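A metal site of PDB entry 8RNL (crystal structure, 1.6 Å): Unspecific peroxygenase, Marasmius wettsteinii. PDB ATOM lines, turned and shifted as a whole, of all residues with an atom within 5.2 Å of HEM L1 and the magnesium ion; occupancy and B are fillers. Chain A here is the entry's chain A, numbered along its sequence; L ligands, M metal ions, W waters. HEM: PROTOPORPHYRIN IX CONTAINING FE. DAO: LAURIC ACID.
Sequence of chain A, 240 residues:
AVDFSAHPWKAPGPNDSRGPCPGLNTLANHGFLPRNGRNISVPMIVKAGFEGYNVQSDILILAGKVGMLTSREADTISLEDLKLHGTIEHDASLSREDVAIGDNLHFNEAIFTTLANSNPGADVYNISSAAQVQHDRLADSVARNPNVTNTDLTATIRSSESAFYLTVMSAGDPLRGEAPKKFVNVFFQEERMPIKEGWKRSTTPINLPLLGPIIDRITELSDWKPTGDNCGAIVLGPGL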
ATOM      1  N   PRO A  20       7.832  -1.944  18.207  1.00  0.00           N
ATOM      2  CA  PRO A  20       8.214  -1.301  16.965  1.00  0.00           C
ATOM      3  C   PRO A  20       8.177   0.232  17.005  1.00  0.00           C
ATOM      4  O   PRO A  20       8.466   0.871  16.005  1.00  0.00           O
ATOM      5  CB  PRO A  20       7.146  -1.850  16.014  1.00  0.00           C
ATOM      6  CG  PRO A  20       5.899  -1.884  16.882  1.00  0.00           C
ATOM      7  CD  PRO A  20       6.412  -2.345  18.238  1.00  0.00           C
ATOM      8  N   CYS A  21       7.821   0.790  18.175  1.00  0.00           N
ATOM      9  CA  CYS A  21       7.642   2.223  18.331  1.00  0.00           C
ATOM     10  C   CYS A  21       8.811   2.853  19.065  1.00  0.00           C
ATOM     11  O   CYS A  21       9.000   2.585  20.249  1.00  0.00           O
ATOM     12  CB  CYS A  21       6.358   2.538  19.084  1.00  0.00           C
ATOM     13  SG  CYS A  21       6.166   4.305  19.439  1.00  0.00           S
ATOM     14  N   PRO A  22       9.622   3.718  18.415  1.00  0.00           N
ATOM     15  CA  PRO A  22      10.726   4.389  19.106  1.00  0.00           C
ATOM     16  C   PRO A  22      10.237   5.330  20.201  1.00  0.00           C
ATOM     17  O   PRO A  22      10.938   5.588  21.193  1.00  0.00           O
ATOM     18  CB  PRO A  22      11.458   5.150  18.001  1.00  0.00           C
ATOM     19  CG  PRO A  22      10.384   5.380  16.949  1.00  0.00           C
ATOM     20  CD  PRO A  22       9.539   4.122  17.007  1.00  0.00           C
ATOM     21  N   GLY A  23       9.044   5.882  20.049  1.00  0.00           N
ATOM     22  CA  GLY A  23       8.514   6.795  21.056  1.00  0.00           C
ATOM     23  C   GLY A  23       8.309   6.108  22.391  1.00  0.00           C
ATOM     24  O   GLY A  23       8.783   6.591  23.432  1.00  0.00           O
ATOM     25  N   LEU A  24       7.600   4.983  22.390  1.00  0.00           N
ATOM     26  CA  LEU A  24       7.317   4.255  23.615  1.00  0.00           C
ATOM     27  C   LEU A  24       8.574   3.566  24.125  1.00  0.00           C
ATOM     28  O   LEU A  24       8.804   3.532  25.332  1.00  0.00           O
ATOM     29  CB  LEU A  24       6.177   3.265  23.391  1.00  0.00           C
ATOM     30  CG  LEU A  24       4.847   3.896  23.003  1.00  0.00           C
ATOM     31  CD1 LEU A  24       3.811   2.807  22.836  1.00  0.00           C
ATOM     32  CD2 LEU A  24       4.380   4.944  24.008  1.00  0.00           C
ATOM     33  N   LEU A  27      10.646   6.090  26.004  1.00  0.00           N
ATOM     34  CA  LEU A  27      10.083   6.381  27.313  1.00  0.00           C
ATOM     35  C   LEU A  27      10.432   5.280  28.296  1.00  0.00           C
ATOM     36  O   LEU A  27      10.745   5.574  29.463  1.00  0.00           O
ATOM     37  CB  LEU A  27       8.572   6.584  27.197  1.00  0.00           C
ATOM     38  CG  LEU A  27       8.148   7.867  26.481  1.00  0.00           C
ATOM     39  CD1 LEU A  27       6.658   7.858  26.225  1.00  0.00           C
ATOM     40  CD2 LEU A  27       8.531   9.127  27.282  1.00  0.00           C
ATOM     41  N   ILE A  45       0.618   5.465  29.551  1.00  0.00           N
ATOM     42  CA  ILE A  45       1.144   6.049  28.331  1.00  0.00           C
ATOM     43  C   ILE A  45       0.878   7.558  28.267  1.00  0.00           C
ATOM     44  O   ILE A  45       1.754   8.334  27.890  1.00  0.00           O
ATOM     45  CB  ILE A  45       0.567   5.323  27.103  1.00  0.00           C
ATOM     46  CG1 ILE A  45       1.072   3.882  27.035  1.00  0.00           C
ATOM     47  CG2 ILE A  45       0.859   6.094  25.837  1.00  0.00           C
ATOM     48  CD1 ILE A  45       0.314   3.019  26.065  1.00  0.00           C
ATOM     49  N   TYR A  53       7.660  14.148  26.659  1.00  0.00           N
ATOM     50  CA  TYR A  53       7.664  14.763  25.349  1.00  0.00           C
ATOM     51  C   TYR A  53       6.714  15.960  25.241  1.00  0.00           C
ATOM     52  O   TYR A  53       6.736  16.662  24.223  1.00  0.00           O
ATOM     53  CB  TYR A  53       7.192  13.744  24.300  1.00  0.00           C
ATOM     54  CG  TYR A  53       7.991  12.474  24.147  1.00  0.00           C
ATOM     55  CD1 TYR A  53       9.380  12.458  24.158  1.00  0.00           C
ATOM     56  CD2 TYR A  53       7.351  11.272  23.892  1.00  0.00           C
ATOM     57  CE1 TYR A  53      10.096  11.294  23.945  1.00  0.00           C
ATOM     58  CE2 TYR A  53       8.059  10.104  23.649  1.00  0.00           C
ATOM     59  CZ  TYR A  53       9.436  10.107  23.687  1.00  0.00           C
ATOM     60  OH  TYR A  53      10.133   8.948  23.485  1.00  0.00           O
ATOM     61  N   VAL A  55       3.591  15.528  24.866  1.00  0.00           N
ATOM     62  CA  VAL A  55       2.517  15.066  23.993  1.00  0.00           C
ATOM     63  C   VAL A  55       1.250  14.920  24.842  1.00  0.00           C
ATOM     64  O   VAL A  55       1.279  14.343  25.928  1.00  0.00           O
ATOM     65  CB  VAL A  55       2.897  13.766  23.265  1.00  0.00           C
ATOM     66  CG1 VAL A  55       1.715  13.183  22.515  1.00  0.00           C
ATOM     67  CG2 VAL A  55       4.060  13.979  22.331  1.00  0.00           C
ATOM     68  N   ILE A  59      -4.082  12.618  21.465  1.00  0.00           N
ATOM     69  CA  ILE A  59      -3.506  11.661  20.526  1.00  0.00           C
ATOM     70  C   ILE A  59      -3.159  10.366  21.270  1.00  0.00           C
ATOM     71  O   ILE A  59      -3.310   9.288  20.710  1.00  0.00           O
ATOM     72  CB  ILE A  59      -2.315  12.238  19.735  1.00  0.00           C
ATOM     73  CG1 ILE A  59      -1.831  11.244  18.668  1.00  0.00           C
ATOM     74  CG2 ILE A  59      -1.181  12.648  20.656  1.00  0.00           C
ATOM     75  CD1 ILE A  59      -0.905  11.817  17.622  1.00  0.00           C
ATOM     76  N   LEU A  60      -2.715  10.454  22.527  1.00  0.00           N
ATOM     77  CA  LEU A  60      -2.267   9.272  23.227  1.00  0.00           C
ATOM     78  C   LEU A  60      -3.423   8.370  23.657  1.00  0.00           C
ATOM     79  O   LEU A  60      -3.266   7.152  23.714  1.00  0.00           O
ATOM     80  CB  LEU A  60      -1.375   9.664  24.403  1.00  0.00           C
ATOM     81  CG  LEU A  60      -0.076  10.362  24.009  1.00  0.00           C
ATOM     82  CD1 LEU A  60       0.719  10.768  25.229  1.00  0.00           C
ATOM     83  CD2 LEU A  60       0.794   9.487  23.092  1.00  0.00           C
ATOM     84  N   ALA A  63      -4.547   6.701  20.088  1.00  0.00           N
ATOM     85  CA  ALA A  63      -3.596   5.693  19.663  1.00  0.00           C
ATOM     86  C   ALA A  63      -3.466   4.579  20.703  1.00  0.00           C
ATOM     87  O   ALA A  63      -3.404   3.403  20.373  1.00  0.00           O
ATOM     88  CB  ALA A  63      -2.259   6.336  19.392  1.00  0.00           C
ATOM     89  N   GLY A  64      -3.416   4.965  21.976  1.00  0.00           N
ATOM     90  CA  GLY A  64      -3.258   4.031  23.073  1.00  0.00           C
ATOM     91  C   GLY A  64      -4.330   2.941  23.086  1.00  0.00           C
ATOM     92  O   GLY A  64      -4.025   1.767  23.281  1.00  0.00           O
ATOM     93  N   GLY A  67      -3.827   0.555  20.418  1.00  0.00           N
ATOM     94  CA  GLY A  67      -2.721  -0.314  20.803  1.00  0.00           C
ATOM     95  C   GLY A  67      -3.103  -1.392  21.806  1.00  0.00           C
ATOM     96  O   GLY A  67      -2.575  -2.487  21.779  1.00  0.00           O
ATOM     97  N   LEU A  82       2.738  -4.599  20.459  1.00  0.00           N
ATOM     98  CA  LEU A  82       2.393  -3.625  19.434  1.00  0.00           C
ATOM     99  C   LEU A  82       2.924  -4.004  18.046  1.00  0.00           C
ATOM    100  O   LEU A  82       2.561  -3.369  17.059  1.00  0.00           O
ATOM    101  CB  LEU A  82       2.950  -2.270  19.859  1.00  0.00           C
ATOM    102  CG  LEU A  82       2.267  -1.635  21.058  1.00  0.00           C
ATOM    103  CD1 LEU A  82       3.028  -0.405  21.495  1.00  0.00           C
ATOM    104  CD2 LEU A  82       0.819  -1.277  20.754  1.00  0.00           C
ATOM    105  N   ILE A  88      -1.871  -1.408  14.437  1.00  0.00           N
ATOM    106  CA  ILE A  88      -1.151  -0.186  14.080  1.00  0.00           C
ATOM    107  C   ILE A  88       0.041  -0.528  13.186  1.00  0.00           C
ATOM    108  O   ILE A  88       0.251   0.149  12.177  1.00  0.00           O
ATOM    109  CB  ILE A  88      -0.715   0.582  15.338  1.00  0.00           C
ATOM    110  CG1 ILE A  88      -1.928   0.999  16.177  1.00  0.00           C
ATOM    111  CG2 ILE A  88       0.119   1.798  14.982  1.00  0.00           C
ATOM    112  CD1 ILE A  88      -1.548   1.536  17.553  1.00  0.00           C
ATOM    113  N   GLU A  89       0.810  -1.557  13.547  1.00  0.00           N
ATOM    114  CA  GLU A  89       2.027  -1.891  12.816  1.00  0.00           C
ATOM    115  C   GLU A  89       1.691  -2.128  11.335  1.00  0.00           C
ATOM    116  O   GLU A  89       0.692  -2.755  10.988  1.00  0.00           O
ATOM    117  CB  GLU A  89       2.715  -3.108  13.434  1.00  0.00           C
ATOM    118  CG  GLU A  89       4.139  -3.301  12.948  1.00  0.00           C
ATOM    119  CD  GLU A  89       4.250  -3.896  11.555  1.00  0.00           C
ATOM    120  OE1 GLU A  89       3.490  -4.865  11.256  1.00  0.00           O
ATOM    121  OE2 GLU A  89       5.107  -3.432  10.798  1.00  0.00           O
ATOM    122  N   HIS A  90       2.546  -1.575  10.483  1.00  0.00           N
ATOM    123  CA  HIS A  90       2.313  -1.483   9.045  1.00  0.00           C
ATOM    124  C   HIS A  90       3.612  -1.669   8.274  1.00  0.00           C
ATOM    125  O   HIS A  90       4.727  -1.478   8.779  1.00  0.00           O
ATOM    126  CB  HIS A  90       1.702  -0.120   8.717  1.00  0.00           C
ATOM    127  CG  HIS A  90       2.505   1.024   9.234  1.00  0.00           C
ATOM    128  ND1 HIS A  90       3.690   1.412   8.665  1.00  0.00           N
ATOM    129  CD2 HIS A  90       2.345   1.816  10.329  1.00  0.00           C
ATOM    130  CE1 HIS A  90       4.222   2.388   9.373  1.00  0.00           C
ATOM    131  NE2 HIS A  90       3.405   2.665  10.386  1.00  0.00           N
ATOM    132  N   ASP A  91       3.441  -1.947   6.977  1.00  0.00           N
ATOM    133  CA  ASP A  91       4.549  -1.982   6.045  1.00  0.00           C
ATOM    134  C   ASP A  91       5.045  -0.563   5.766  1.00  0.00           C
ATOM    135  O   ASP A  91       4.397   0.420   6.115  1.00  0.00           O
ATOM    136  CB  ASP A  91       4.093  -2.634   4.733  1.00  0.00           C
ATOM    137  CG  ASP A  91       3.631  -4.069   4.911  1.00  0.00           C
ATOM    138  OD1 ASP A  91       4.149  -4.746   5.799  1.00  0.00           O
ATOM    139  OD2 ASP A  91       2.761  -4.505   4.108  1.00  0.00           O
ATOM    140  N   SER A  93       7.600   0.966   7.076  1.00  0.00           N
ATOM    141  CA  SER A  93       8.105   1.666   8.246  1.00  0.00           C
ATOM    142  C   SER A  93       9.416   2.382   7.912  1.00  0.00           C
ATOM    143  O   SER A  93      10.065   2.064   6.931  1.00  0.00           O
ATOM    144  CB  SER A  93       8.329   0.692   9.385  1.00  0.00           C
ATOM    145  OG  SER A  93       7.090   0.176   9.863  1.00  0.00           O
ATOM    146  N   LEU A  94       9.806   3.332   8.765  1.00  0.00           N
ATOM    147  CA  LEU A  94      10.998   4.144   8.566  1.00  0.00           C
ATOM    148  C   LEU A  94      12.275   3.415   9.001  1.00  0.00           C
ATOM    149  O   LEU A  94      13.344   3.785   8.545  1.00  0.00           O
ATOM    150  CB  LEU A  94      10.861   5.421   9.400  1.00  0.00           C
ATOM    151  CG  LEU A  94       9.661   6.305   9.046  1.00  0.00           C
ATOM    152  CD1 LEU A  94       9.390   7.315  10.156  1.00  0.00           C
ATOM    153  CD2 LEU A  94       9.862   7.013   7.733  1.00  0.00           C
ATOM    154  N   SER A  95      12.150   2.444   9.911  1.00  0.00           N
ATOM    155  CA  SER A  95      13.311   1.861  10.575  1.00  0.00           C
ATOM    156  C   SER A  95      13.155   0.359  10.842  1.00  0.00           C
ATOM    157  O   SER A  95      14.041  -0.230  11.451  1.00  0.00           O
ATOM    158  CB  SER A  95      13.616   2.621  11.857  1.00  0.00           C
ATOM    159  OG  SER A  95      12.654   2.361  12.882  1.00  0.00           O
ATOM    160  N   ARG A  96      12.041  -0.236  10.416  1.00  0.00           N
ATOM    161  CA  ARG A  96      11.755  -1.660  10.564  1.00  0.00           C
ATOM    162  C   ARG A  96      11.467  -2.243   9.177  1.00  0.00           C
ATOM    163  O   ARG A  96      11.107  -1.507   8.271  1.00  0.00           O
ATOM    164  CB  ARG A  96      10.537  -1.913  11.458  1.00  0.00           C
ATOM    165  CG  ARG A  96      10.809  -2.001  12.955  1.00  0.00           C
ATOM    166  CD  ARG A  96      11.465  -0.783  13.558  1.00  0.00           C
ATOM    167  NE  ARG A  96      11.503  -0.915  15.008  1.00  0.00           N
ATOM    168  CZ  ARG A  96      12.078  -0.055  15.840  1.00  0.00           C
ATOM    169  NH1 ARG A  96      12.636   1.059  15.406  1.00  0.00           N
ATOM    170  NH2 ARG A  96      12.100  -0.359  17.127  1.00  0.00           N
ATOM    171  N   GLU A  97      11.602  -3.571   9.071  1.00  0.00           N
ATOM    172  CA  GLU A  97      11.292  -4.277   7.839  1.00  0.00           C
ATOM    173  C   GLU A  97       9.810  -4.657   7.843  1.00  0.00           C
ATOM    174  O   GLU A  97       9.189  -4.746   8.887  1.00  0.00           O
ATOM    175  CB  GLU A  97      12.177  -5.531   7.688  1.00  0.00           C
ATOM    176  CG  GLU A  97      13.664  -5.221   7.735  1.00  0.00           C
ATOM    177  CD  GLU A  97      14.563  -6.453   7.703  1.00  0.00           C
ATOM    178  OE1 GLU A  97      14.214  -7.478   8.345  1.00  0.00           O
ATOM    179  OE2 GLU A  97      15.635  -6.376   7.067  1.00  0.00           O
ATOM    180  N   ASN A 104       9.691  -7.031  11.737  1.00  0.00           N
ATOM    181  CA  ASN A 104       8.868  -5.835  11.827  1.00  0.00           C
ATOM    182  C   ASN A 104       8.964  -5.187  13.197  1.00  0.00           C
ATOM    183  O   ASN A 104       8.202  -4.275  13.479  1.00  0.00           O
ATOM    184  CB  ASN A 104       7.409  -6.113  11.476  1.00  0.00           C
ATOM    185  CG  ASN A 104       6.655  -6.861  12.556  1.00  0.00           C
ATOM    186  OD1 ASN A 104       7.260  -7.502  13.404  1.00  0.00           O
ATOM    187  ND2 ASN A 104       5.336  -6.769  12.566  1.00  0.00           N
ATOM    188  N   GLU A 161       3.351   9.260  12.303  1.00  0.00           N
ATOM    189  CA  GLU A 161       4.638   8.858  12.877  1.00  0.00           C
ATOM    190  C   GLU A 161       5.749   9.821  12.461  1.00  0.00           C
ATOM    191  O   GLU A 161       6.608  10.191  13.276  1.00  0.00           O
ATOM    192  CB  GLU A 161       4.889   7.394  12.527  1.00  0.00           C
ATOM    193  CG  GLU A 161       3.902   6.500  13.272  1.00  0.00           C
ATOM    194  CD  GLU A 161       3.642   5.097  12.769  1.00  0.00           C
ATOM    195  OE1 GLU A 161       4.151   4.742  11.716  1.00  0.00           O
ATOM    196  OE2 GLU A 161       2.871   4.383  13.463  1.00  0.00           O
ATOM    197  N   SER A 162       5.775  10.246  11.198  1.00  0.00           N
ATOM    198  CA  SER A 162       6.749  11.227  10.754  1.00  0.00           C
ATOM    199  C   SER A 162       6.547  12.552  11.496  1.00  0.00           C
ATOM    200  O   SER A 162       7.516  13.165  11.937  1.00  0.00           O
ATOM    201  CB  SER A 162       6.725  11.413   9.257  1.00  0.00           C
ATOM    202  OG  SER A 162       7.120  10.206   8.604  1.00  0.00           O
ATOM    203  N   PHE A 164       5.404  12.884  14.419  1.00  0.00           N
ATOM    204  CA  PHE A 164       5.887  12.676  15.777  1.00  0.00           C
ATOM    205  C   PHE A 164       7.385  12.963  15.884  1.00  0.00           C
ATOM    206  O   PHE A 164       7.833  13.682  16.783  1.00  0.00           O
ATOM    207  CB  PHE A 164       5.584  11.257  16.261  1.00  0.00           C
ATOM    208  CG  PHE A 164       4.353  11.101  17.103  1.00  0.00           C
ATOM    209  CD1 PHE A 164       4.036  12.067  18.058  1.00  0.00           C
ATOM    210  CD2 PHE A 164       3.616   9.923  17.060  1.00  0.00           C
ATOM    211  CE1 PHE A 164       2.941  11.890  18.891  1.00  0.00           C
ATOM    212  CE2 PHE A 164       2.524   9.758  17.901  1.00  0.00           C
ATOM    213  CZ  PHE A 164       2.183  10.744  18.794  1.00  0.00           C
ATOM    214  N   TYR A 165       8.208  12.370  15.009  1.00  0.00           N
ATOM    215  CA  TYR A 165       9.635  12.596  15.188  1.00  0.00           C
ATOM    216  C   TYR A 165      10.029  14.044  14.881  1.00  0.00           C
ATOM    217  O   TYR A 165      10.918  14.573  15.551  1.00  0.00           O
ATOM    218  CB  TYR A 165      10.517  11.569  14.460  1.00  0.00           C
ATOM    219  CG  TYR A 165      10.676  11.718  12.978  1.00  0.00           C
ATOM    220  CD1 TYR A 165      11.434  12.729  12.397  1.00  0.00           C
ATOM    221  CD2 TYR A 165      10.092  10.802  12.130  1.00  0.00           C
ATOM    222  CE1 TYR A 165      11.593  12.832  11.023  1.00  0.00           C
ATOM    223  CE2 TYR A 165      10.237  10.881  10.760  1.00  0.00           C
ATOM    224  CZ  TYR A 165      10.975  11.896  10.190  1.00  0.00           C
ATOM    225  OH  TYR A 165      11.150  12.047   8.819  1.00  0.00           O
ATOM    226  N   VAL A 168       8.476  15.889  18.375  1.00  0.00           N
ATOM    227  CA  VAL A 168       8.929  15.533  19.705  1.00  0.00           C
ATOM    228  C   VAL A 168      10.430  15.781  19.856  1.00  0.00           C
ATOM    229  O   VAL A 168      10.890  16.107  20.958  1.00  0.00           O
ATOM    230  CB  VAL A 168       8.540  14.089  20.056  1.00  0.00           C
ATOM    231  CG1 VAL A 168       9.206  13.608  21.321  1.00  0.00           C
ATOM    232  CG2 VAL A 168       7.031  13.927  20.143  1.00  0.00           C
ATOM    233  N   PHE A 187      17.320   9.256  18.617  1.00  0.00           N
ATOM    234  CA  PHE A 187      15.996   8.767  18.949  1.00  0.00           C
ATOM    235  C   PHE A 187      15.765   7.398  18.322  1.00  0.00           C
ATOM    236  O   PHE A 187      15.349   6.459  19.008  1.00  0.00           O
ATOM    237  CB  PHE A 187      14.975   9.830  18.545  1.00  0.00           C
ATOM    238  CG  PHE A 187      13.525   9.471  18.729  1.00  0.00           C
ATOM    239  CD1 PHE A 187      12.979   9.366  19.997  1.00  0.00           C
ATOM    240  CD2 PHE A 187      12.696   9.251  17.639  1.00  0.00           C
ATOM    241  CE1 PHE A 187      11.635   9.030  20.181  1.00  0.00           C
ATOM    242  CE2 PHE A 187      11.362   8.951  17.832  1.00  0.00           C
ATOM    243  CZ  PHE A 187      10.829   8.828  19.096  1.00  0.00           C
ATOM    244  N   PHE A 188      16.012   7.260  17.016  1.00  0.00           N
ATOM    245  CA  PHE A 188      15.776   6.000  16.316  1.00  0.00           C
ATOM    246  C   PHE A 188      16.853   4.960  16.630  1.00  0.00           C
ATOM    247  O   PHE A 188      16.535   3.807  16.910  1.00  0.00           O
ATOM    248  CB  PHE A 188      15.727   6.229  14.799  1.00  0.00           C
ATOM    249  CG  PHE A 188      14.383   6.657  14.242  1.00  0.00           C
ATOM    250  CD1 PHE A 188      13.423   5.729  13.925  1.00  0.00           C
ATOM    251  CD2 PHE A 188      14.078   8.000  14.076  1.00  0.00           C
ATOM    252  CE1 PHE A 188      12.203   6.124  13.407  1.00  0.00           C
ATOM    253  CE2 PHE A 188      12.855   8.395  13.572  1.00  0.00           C
ATOM    254  CZ  PHE A 188      11.918   7.441  13.223  1.00  0.00           C
HETATM  255  CHA HEM L   1       5.697   3.631  15.226  1.00  0.00           C
HETATM  256  CHB HEM L   1       2.357   2.617  18.527  1.00  0.00           C
HETATM  257  CHC HEM L   1       3.196   6.879  20.639  1.00  0.00           C
HETATM  258  CHD HEM L   1       6.700   7.763  17.450  1.00  0.00           C
HETATM  259  C1A HEM L   1       4.771   2.988  15.976  1.00  0.00           C
HETATM  260  C2A HEM L   1       4.286   1.677  15.724  1.00  0.00           C
HETATM  261  C3A HEM L   1       3.359   1.358  16.633  1.00  0.00           C
HETATM  262  C4A HEM L   1       3.234   2.514  17.491  1.00  0.00           C
HETATM  263  CMA HEM L   1       2.618   0.050  16.712  1.00  0.00           C
HETATM  264  CAA HEM L   1       4.787   0.780  14.610  1.00  0.00           C
HETATM  265  CBA HEM L   1       4.227   1.236  13.237  1.00  0.00           C
HETATM  266  CGA HEM L   1       5.138   0.782  12.113  1.00  0.00           C
HETATM  267  O1A HEM L   1       4.877  -0.313  11.495  1.00  0.00           O
HETATM  268  O2A HEM L   1       6.184   1.427  11.820  1.00  0.00           O
HETATM  269  C1B HEM L   1       2.266   3.730  19.362  1.00  0.00           C
HETATM  270  C2B HEM L   1       1.267   3.827  20.403  1.00  0.00           C
HETATM  271  C3B HEM L   1       1.507   5.010  21.024  1.00  0.00           C
HETATM  272  C4B HEM L   1       2.647   5.649  20.309  1.00  0.00           C
HETATM  273  CMB HEM L   1       0.250   2.807  20.787  1.00  0.00           C
HETATM  274  CAB HEM L   1       0.655   5.543  22.102  1.00  0.00           C
HETATM  275  CBB HEM L   1       0.274   6.770  21.978  1.00  0.00           C
HETATM  276  C1C HEM L   1       4.283   7.467  20.043  1.00  0.00           C
HETATM  277  C2C HEM L   1       4.942   8.622  20.467  1.00  0.00           C
HETATM  278  C3C HEM L   1       5.947   8.862  19.566  1.00  0.00           C
HETATM  279  C4C HEM L   1       5.902   7.862  18.545  1.00  0.00           C
HETATM  280  CMC HEM L   1       4.631   9.430  21.726  1.00  0.00           C
HETATM  281  CAC HEM L   1       6.857  10.026  19.708  1.00  0.00           C
HETATM  282  CBC HEM L   1       7.788  10.382  18.872  1.00  0.00           C
HETATM  283  C1D HEM L   1       6.673   6.701  16.518  1.00  0.00           C
HETATM  284  C2D HEM L   1       7.518   6.724  15.289  1.00  0.00           C
HETATM  285  C3D HEM L   1       7.233   5.528  14.688  1.00  0.00           C
HETATM  286  C4D HEM L   1       6.229   4.877  15.537  1.00  0.00           C
HETATM  287  CMD HEM L   1       8.474   7.784  14.849  1.00  0.00           C
HETATM  288  CAD HEM L   1       7.736   5.017  13.352  1.00  0.00           C
HETATM  289  CBD HEM L   1       8.771   3.929  13.427  1.00  0.00           C
HETATM  290  CGD HEM L   1       9.151   3.460  12.038  1.00  0.00           C
HETATM  291  O1D HEM L   1       8.407   3.788  11.067  1.00  0.00           O
HETATM  292  O2D HEM L   1      10.164   2.742  11.922  1.00  0.00           O
HETATM  293  NA  HEM L   1       4.067   3.483  17.055  1.00  0.00           N
HETATM  294  NB  HEM L   1       3.025   4.816  19.330  1.00  0.00           N
HETATM  295  NC  HEM L   1       4.894   7.034  18.910  1.00  0.00           N
HETATM  296  ND  HEM L   1       5.887   5.602  16.632  1.00  0.00           N
HETATM  297 FE   HEM L   1       4.595   5.176  18.016  1.00  0.00          FE
HETATM  298  O1  DAO L   2       2.965   6.138  16.667  1.00  0.00           O
HETATM  299  O2  DAO L   2       1.515   5.051  15.393  1.00  0.00           O
HETATM  300  C1  DAO L   2       1.839   6.052  16.044  1.00  0.00           C
HETATM  301  C2  DAO L   2       0.867   7.228  16.040  1.00  0.00           C
HETATM  302  C3  DAO L   2      -0.443   6.994  15.293  1.00  0.00           C
HETATM  303  C4  DAO L   2      -1.499   6.294  16.140  1.00  0.00           C
HETATM  304  C5  DAO L   2      -2.539   5.472  15.374  1.00  0.00           C
HETATM  305  C6  DAO L   2      -3.982   5.776  15.734  1.00  0.00           C
HETATM  306  C7  DAO L   2      -4.855   6.254  14.601  1.00  0.00           C
HETATM  307  C8  DAO L   2      -4.330   7.464  13.837  1.00  0.00           C
HETATM  308  C9  DAO L   2      -4.354   8.762  14.607  1.00  0.00           C
HETATM  309  C10 DAO L   2      -4.029   9.978  13.774  1.00  0.00           C
HETATM  310  C11 DAO L   2      -5.148  10.456  12.880  1.00  0.00           C
HETATM  311  C12 DAO L   2      -5.045  11.914  12.501  1.00  0.00           C
HETATM  312 MG    MG M   1       6.079  -1.651  10.391  1.00  0.00          MG
HETATM  313  O   HOH W   1       8.337   0.210  13.352  1.00  0.00           O
HETATM  314  O   HOH W   2       7.258  -1.966  12.113  1.00  0.00           O
HETATM  315  O   HOH W   3       6.271   4.858   9.949  1.00  0.00           O
HETATM  316  O   HOH W   4       7.379  -2.656   9.092  1.00  0.00           O
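O1A of HEM L1 lies close to N of His 90, 2.8 Å away. NE2 of His 90 lies close to O2A of HEM L1 (3.4 Å). The side-chain sulfur (SG) of Cys 21 is bound to an iron atom (FE) of HEM L1, 2.3 Å away. The backbone NH (N) of Ser 95 sits at hydrogen-bond distance from an oxygen (O2D) of HEM L1 (2.8 Å). The side-chain hydroxyl (OG) of Ser 95 is in hydrogen-bond range of an oxygen (O2D) of HEM L1, 2.7 Å away. N of Leu 94 lies within hydrogen-bond range of O1D of HEM L1. The side-chain carboxylate of Glu 161 sits close to an oxygen (O2) of DAO L2 (2.5 Å).
An oxygen (O1) of DAO L2 is bound to an iron atom (FE) of HEM L1 (2.3 Å).
OE1 of Glu 89 lies within hydrogen-bond range of ND2 of Asn 104, 3.0 Å away. A ring nitrogen (NE2) of His 90 sits at hydrogen-bond distance from the side-chain carboxylate (OE1) of Glu 161 (2.6 Å). The side-chain sulfur of Cys 21 lies close to the backbone NH of Gly 23 (3.3 Å). The side-chain sulfur of Cys 21 sits close to the backbone NH of Leu 24, at 3.4 Å. The side-chain hydroxyl (OG) of Ser 95 lies within hydrogen-bond range of the guanidinium group (NH1) of Arg 96, 2.8 Å away. The side-chain hydroxyl of Tyr 53 is in hydrogen-bond range of the backbone carbonyl oxygen of Gly 23, 2.7 Å away.
Water W3 bridges O1D of HEM L1 (2.6 Å) and OE1 of Glu 161 (2.8 Å). Water W1 lies within hydrogen-bond range of O of Pro 20 and O2A of HEM L1.
The magnesium ion is bound by the side-chain carboxylate (OE2) of Glu 89, at 2.1 Å. Water W4 is bound to the magnesium ion, at 2.1 Å. Water W2 binds the magnesium ion (2.1 Å). The magnesium ion is bound by an oxygen (O1A) of HEM L1 (2.1 Å). O of His 90 is bound to the magnesium ion, 2.1 Å away. The magnesium ion is bound by the side-chain hydroxyl (OG) of Ser 93, at 2.2 Å.
Pro 20 touches HEM L1. Pro 22 touches HEM L1. Gly 23 touches HEM L1 (CA to C3C, 3.6 Å). Leu 24 touches HEM L1. CG2 of Ile 45 touches CAB of HEM L1, 3.8 Å away. Tyr 53 touches HEM L1. Leu 60 touches HEM L1 (CD2 to CBB, 3.0 Å). Ala 63 touches HEM L1. Leu 82 touches HEM L1 (O to CMA, 3.4 Å). CG2 of Ile 88 touches CMA of HEM L1, 3.5 Å away. Arg 96 touches HEM L1. Glu 161 touches HEM L1. CD2 of Phe 164 touches C4C of HEM L1, at 3.4 Å. Val 168 touches HEM L1 (CG2 to CBC, 3.8 Å). Phe 187 touches HEM L1 (CZ to CBC, 3.4 Å). Phe 188 touches HEM L1. Hydrophobic or aromatic side chains within 4 Å of HEM L1: Pro 20, Pro 22, Leu 24, Ile 45, Tyr 53, Leu 60, Ala 63, Leu 82, Ile 88, His 90, Leu 94, Phe 164, Val 168, Phe 187 and Phe 188. Along chain A the residues within 4 Å of HEM L1 span positions 20 to 188. The nearest printed residue that does not touch HEM L1 is Gly 64 (4.1 Å).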
